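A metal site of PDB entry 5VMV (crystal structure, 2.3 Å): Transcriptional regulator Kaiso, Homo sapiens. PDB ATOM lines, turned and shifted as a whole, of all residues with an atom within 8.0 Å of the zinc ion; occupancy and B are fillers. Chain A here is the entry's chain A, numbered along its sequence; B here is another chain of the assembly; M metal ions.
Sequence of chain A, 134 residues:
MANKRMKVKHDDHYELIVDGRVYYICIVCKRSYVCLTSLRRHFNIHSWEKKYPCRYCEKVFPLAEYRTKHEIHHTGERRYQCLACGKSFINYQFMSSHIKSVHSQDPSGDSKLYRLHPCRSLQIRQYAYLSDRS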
ATOM      1  N   ASP A  12      13.403  20.473  10.269  1.00  0.00           N
ATOM      2  CA  ASP A  12      14.491  20.029   9.405  1.00  0.00           C
ATOM      3  C   ASP A  12      14.006  18.927   8.464  1.00  0.00           C
ATOM      4  O   ASP A  12      14.684  18.569   7.503  1.00  0.00           O
ATOM      5  CB  ASP A  12      15.694  19.559  10.244  1.00  0.00           C
ATOM      6  CG  ASP A  12      15.345  18.403  11.166  1.00  0.00           C
ATOM      7  OD1 ASP A  12      14.149  18.182  11.435  1.00  0.00           O
ATOM      8  OD2 ASP A  12      16.279  17.726  11.649  1.00  0.00           O
ATOM      9  N   ILE A  25      11.856  12.778   5.442  1.00  0.00           N
ATOM     10  CA  ILE A  25      12.472  13.437   4.294  1.00  0.00           C
ATOM     11  C   ILE A  25      13.176  14.718   4.716  1.00  0.00           C
ATOM     12  O   ILE A  25      12.592  15.580   5.391  1.00  0.00           O
ATOM     13  CB  ILE A  25      11.426  13.780   3.181  1.00  0.00           C
ATOM     14  CG1 ILE A  25      11.146  12.601   2.248  1.00  0.00           C
ATOM     15  CG2 ILE A  25      11.976  14.862   2.289  1.00  0.00           C
ATOM     16  CD1 ILE A  25      10.668  11.334   2.911  1.00  0.00           C
ATOM     17  N   CYS A  26      14.442  14.837   4.316  1.00  0.00           N
ATOM     18  CA  CYS A  26      15.244  16.026   4.567  1.00  0.00           C
ATOM     19  C   CYS A  26      14.722  17.239   3.779  1.00  0.00           C
ATOM     20  O   CYS A  26      14.681  17.183   2.554  1.00  0.00           O
ATOM     21  CB  CYS A  26      16.693  15.729   4.184  1.00  0.00           C
ATOM     22  SG  CYS A  26      17.822  17.081   4.444  1.00  0.00           S
ATOM     23  N   ILE A  27      14.348  18.327   4.466  1.00  0.00           N
ATOM     24  CA  ILE A  27      13.738  19.468   3.751  1.00  0.00           C
ATOM     25  C   ILE A  27      14.700  20.109   2.751  1.00  0.00           C
ATOM     26  O   ILE A  27      14.257  20.697   1.756  1.00  0.00           O
ATOM     27  CB  ILE A  27      13.214  20.599   4.696  1.00  0.00           C
ATOM     28  CG1 ILE A  27      14.297  21.085   5.656  1.00  0.00           C
ATOM     29  CG2 ILE A  27      11.970  20.158   5.465  1.00  0.00           C
ATOM     30  CD1 ILE A  27      13.864  22.289   6.460  1.00  0.00           C
ATOM     31  N   VAL A  28      15.999  20.018   3.018  1.00  0.00           N
ATOM     32  CA  VAL A  28      17.001  20.629   2.141  1.00  0.00           C
ATOM     33  C   VAL A  28      17.221  19.828   0.853  1.00  0.00           C
ATOM     34  O   VAL A  28      17.115  20.395  -0.240  1.00  0.00           O
ATOM     35  CB  VAL A  28      18.351  20.801   2.870  1.00  0.00           C
ATOM     36  CG1 VAL A  28      19.460  21.167   1.875  1.00  0.00           C
ATOM     37  CG2 VAL A  28      18.243  21.850   3.962  1.00  0.00           C
ATOM     38  N   CYS A  29      17.545  18.538   0.959  1.00  0.00           N
ATOM     39  CA  CYS A  29      17.889  17.753  -0.233  1.00  0.00           C
ATOM     40  C   CYS A  29      16.866  16.661  -0.573  1.00  0.00           C
ATOM     41  O   CYS A  29      17.098  15.828  -1.453  1.00  0.00           O
ATOM     42  CB  CYS A  29      19.295  17.134  -0.058  1.00  0.00           C
ATOM     43  SG  CYS A  29      19.474  15.827   1.176  1.00  0.00           S
ATOM     44  N   LYS A  30      15.711  16.705   0.097  1.00  0.00           N
ATOM     45  CA  LYS A  30      14.618  15.740  -0.092  1.00  0.00           C
ATOM     46  C   LYS A  30      15.039  14.273  -0.015  1.00  0.00           C
ATOM     47  O   LYS A  30      14.410  13.422  -0.644  1.00  0.00           O
ATOM     48  CB  LYS A  30      13.889  15.954  -1.429  1.00  0.00           C
ATOM     49  CG  LYS A  30      14.140  17.267  -2.201  1.00  0.00           C
ATOM     50  CD  LYS A  30      13.600  18.514  -1.499  1.00  0.00           C
ATOM     51  CE  LYS A  30      14.325  19.774  -2.031  1.00  0.00           C
ATOM     52  NZ  LYS A  30      13.910  21.046  -1.378  1.00  0.00           N
ATOM     53  N   ARG A  31      16.070  13.946   0.762  1.00  0.00           N
ATOM     54  CA  ARG A  31      16.475  12.543   0.878  1.00  0.00           C
ATOM     55  C   ARG A  31      15.606  11.782   1.865  1.00  0.00           C
ATOM     56  O   ARG A  31      15.151  12.340   2.870  1.00  0.00           O
ATOM     57  CB  ARG A  31      17.924  12.413   1.290  1.00  0.00           C
ATOM     58  CG  ARG A  31      18.877  12.244   0.152  1.00  0.00           C
ATOM     59  CD  ARG A  31      20.184  11.725   0.698  1.00  0.00           C
ATOM     60  NE  ARG A  31      21.321  12.116  -0.126  1.00  0.00           N
ATOM     61  CZ  ARG A  31      22.000  11.279  -0.886  1.00  0.00           C
ATOM     62  NH1 ARG A  31      21.660   9.987  -0.930  1.00  0.00           N
ATOM     63  NH2 ARG A  31      23.025  11.719  -1.605  1.00  0.00           N
ATOM     64  N   SER A  32      15.424  10.501   1.574  1.00  0.00           N
ATOM     65  CA  SER A  32      14.496   9.638   2.291  1.00  0.00           C
ATOM     66  C   SER A  32      15.184   8.825   3.376  1.00  0.00           C
ATOM     67  O   SER A  32      16.239   8.226   3.146  1.00  0.00           O
ATOM     68  CB  SER A  32      13.803   8.718   1.297  1.00  0.00           C
ATOM     69  OG  SER A  32      12.894   7.865   1.958  1.00  0.00           O
ATOM     70  N   TYR A  33      14.592   8.781   4.568  1.00  0.00           N
ATOM     71  CA  TYR A  33      15.199   8.053   5.669  1.00  0.00           C
ATOM     72  C   TYR A  33      14.171   7.265   6.460  1.00  0.00           C
ATOM     73  O   TYR A  33      13.131   7.795   6.857  1.00  0.00           O
ATOM     74  CB  TYR A  33      15.953   9.026   6.606  1.00  0.00           C
ATOM     75  CG  TYR A  33      17.171   9.647   5.946  1.00  0.00           C
ATOM     76  CD1 TYR A  33      17.072  10.856   5.278  1.00  0.00           C
ATOM     77  CD2 TYR A  33      18.418   8.998   5.970  1.00  0.00           C
ATOM     78  CE1 TYR A  33      18.156  11.435   4.658  1.00  0.00           C
ATOM     79  CE2 TYR A  33      19.531   9.565   5.346  1.00  0.00           C
ATOM     80  CZ  TYR A  33      19.375  10.783   4.691  1.00  0.00           C
ATOM     81  OH  TYR A  33      20.438  11.383   4.057  1.00  0.00           O
ATOM     82  N   LEU A  39      18.315  10.575   9.682  1.00  0.00           N
ATOM     83  CA  LEU A  39      18.091  11.865   9.056  1.00  0.00           C
ATOM     84  C   LEU A  39      18.857  12.966   9.766  1.00  0.00           C
ATOM     85  O   LEU A  39      19.451  13.807   9.109  1.00  0.00           O
ATOM     86  CB  LEU A  39      16.596  12.218   8.977  1.00  0.00           C
ATOM     87  CG  LEU A  39      16.390  13.628   8.413  1.00  0.00           C
ATOM     88  CD1 LEU A  39      15.279  13.679   7.375  1.00  0.00           C
ATOM     89  CD2 LEU A  39      16.143  14.613   9.547  1.00  0.00           C
ATOM     90  N   HIS A  42      22.446  12.833   8.978  1.00  0.00           N
ATOM     91  CA  HIS A  42      22.614  13.425   7.660  1.00  0.00           C
ATOM     92  C   HIS A  42      22.537  14.963   7.626  1.00  0.00           C
ATOM     93  O   HIS A  42      23.377  15.623   7.027  1.00  0.00           O
ATOM     94  CB  HIS A  42      21.580  12.841   6.734  1.00  0.00           C
ATOM     95  CG  HIS A  42      21.330  13.684   5.524  1.00  0.00           C
ATOM     96  ND1 HIS A  42      22.166  13.687   4.439  1.00  0.00           N
ATOM     97  CD2 HIS A  42      20.348  14.579   5.257  1.00  0.00           C
ATOM     98  CE1 HIS A  42      21.706  14.536   3.539  1.00  0.00           C
ATOM     99  NE2 HIS A  42      20.607  15.092   4.010  1.00  0.00           N
ATOM    100  N   PHE A  43      21.523  15.532   8.256  1.00  0.00           N
ATOM    101  CA  PHE A  43      21.195  16.955   8.124  1.00  0.00           C
ATOM    102  C   PHE A  43      22.305  17.805   8.729  1.00  0.00           C
ATOM    103  O   PHE A  43      22.462  19.010   8.395  1.00  0.00           O
ATOM    104  CB  PHE A  43      19.866  17.249   8.792  1.00  0.00           C
ATOM    105  CG  PHE A  43      19.276  18.595   8.446  1.00  0.00           C
ATOM    106  CD1 PHE A  43      18.458  18.733   7.341  1.00  0.00           C
ATOM    107  CD2 PHE A  43      19.541  19.703   9.232  1.00  0.00           C
ATOM    108  CE1 PHE A  43      17.901  19.970   7.018  1.00  0.00           C
ATOM    109  CE2 PHE A  43      18.992  20.935   8.911  1.00  0.00           C
ATOM    110  CZ  PHE A  43      18.174  21.072   7.806  1.00  0.00           C
ATOM    111  N   ASN A  44      23.096  17.184   9.594  1.00  0.00           N
ATOM    112  CA  ASN A  44      24.216  17.933  10.121  1.00  0.00           C
ATOM    113  C   ASN A  44      25.162  18.363   8.995  1.00  0.00           C
ATOM    114  O   ASN A  44      25.880  19.354   9.137  1.00  0.00           O
ATOM    115  CB  ASN A  44      24.985  17.137  11.168  1.00  0.00           C
ATOM    116  CG  ASN A  44      25.936  18.012  11.963  1.00  0.00           C
ATOM    117  OD1 ASN A  44      25.569  19.103  12.401  1.00  0.00           O
ATOM    118  ND2 ASN A  44      27.158  17.540  12.142  1.00  0.00           N
ATOM    119  N   ILE A  45      25.141  17.669   7.853  1.00  0.00           N
ATOM    120  CA  ILE A  45      26.006  18.056   6.744  1.00  0.00           C
ATOM    121  C   ILE A  45      25.486  19.323   6.056  1.00  0.00           C
ATOM    122  O   ILE A  45      26.235  19.999   5.365  1.00  0.00           O
ATOM    123  CB  ILE A  45      26.173  16.911   5.713  1.00  0.00           C
ATOM    124  CG1 ILE A  45      27.481  17.097   4.929  1.00  0.00           C
ATOM    125  CG2 ILE A  45      25.030  16.830   4.754  1.00  0.00           C
ATOM    126  CD1 ILE A  45      27.571  16.246   3.690  1.00  0.00           C
ATOM    127  N   HIS A  46      24.210  19.640   6.271  1.00  0.00           N
ATOM    128  CA  HIS A  46      23.625  20.891   5.779  1.00  0.00           C
ATOM    129  C   HIS A  46      23.837  22.026   6.782  1.00  0.00           C
ATOM    130  O   HIS A  46      24.189  23.142   6.400  1.00  0.00           O
ATOM    131  CB  HIS A  46      22.116  20.739   5.505  1.00  0.00           C
ATOM    132  CG  HIS A  46      21.789  19.697   4.472  1.00  0.00           C
ATOM    133  ND1 HIS A  46      22.455  19.607   3.266  1.00  0.00           N
ATOM    134  CD2 HIS A  46      20.862  18.711   4.467  1.00  0.00           C
ATOM    135  CE1 HIS A  46      21.947  18.604   2.568  1.00  0.00           C
ATOM    136  NE2 HIS A  46      20.983  18.049   3.274  1.00  0.00           N
ATOM    137  N1  5CM B   8      23.598   4.697   6.472  1.00  0.00           N
ATOM    138  C2  5CM B   8      24.363   3.425   6.405  1.00  0.00           C
ATOM    139  N3  5CM B   8      25.823   3.442   6.713  1.00  0.00           N
ATOM    140  C4  5CM B   8      26.500   4.647   7.028  1.00  0.00           C
ATOM    141  C5  5CM B   8      25.726   5.928   7.107  1.00  0.00           C
ATOM    142  C5A 5CM B   8      26.429   7.239   7.459  1.00  0.00           C
ATOM    143  C6  5CM B   8      24.275   5.928   6.808  1.00  0.00           C
ATOM    144  O2  5CM B   8      23.807   2.425   6.112  1.00  0.00           O
ATOM    145  N4  5CM B   8      27.918   4.574   7.309  1.00  0.00           N
ATOM    146  C1' 5CM B   8      22.174   4.624   6.161  1.00  0.00           C
ATOM    147  C2' 5CM B   8      21.340   5.939   6.454  1.00  0.00           C
ATOM    148  C3' 5CM B   8      20.138   5.603   5.609  1.00  0.00           C
ATOM    149  C4' 5CM B   8      20.615   5.052   4.466  1.00  0.00           C
ATOM    150  O4' 5CM B   8      22.066   4.502   4.870  1.00  0.00           O
ATOM    151  O3' 5CM B   8      19.471   4.518   6.354  1.00  0.00           O
ATOM    152  C5' 5CM B   8      20.751   6.028   3.350  1.00  0.00           C
ATOM    153  O5' 5CM B   8      21.292   7.243   3.815  1.00  0.00           O
ATOM    154  P   5CM B   8      21.681   8.332   2.668  1.00  0.00           P
ATOM    155  OP1 5CM B   8      20.528   8.631   1.746  1.00  0.00           O
ATOM    156  OP2 5CM B   8      22.335   9.552   3.301  1.00  0.00           O
HETATM  157 ZN    ZN M   1      19.682  16.610   3.205  1.00  0.00          ZN
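Within 4 Å of the zinc ion: Cys 26, Cys 29, His 42 and His 46.
The nearest printed residue that does not touch the zinc ion is Val 28 (4.4 Å).
OH of Tyr 33 lies close to ND1 of His 42 (2.9 Å).
The backbone carbonyl oxygen (O) of Arg 31 sits at hydrogen-bond distance from the backbone NH (N) of Cys 26, at 3.0 Å.
The side-chain sulfur (SG) of Cys 26 lies close to the backbone NH (N) of Val 28 (3.7 Å).
The zinc ion is bound by a ring nitrogen (NE2) of His 46 (1.9 Å), a ring nitrogen (NE2) of His 42 (2.0 Å), the side-chain sulfur (SG) of Cys 29 (2.2 Å) and the side-chain sulfur (SG) of Cys 26 (2.3 Å).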
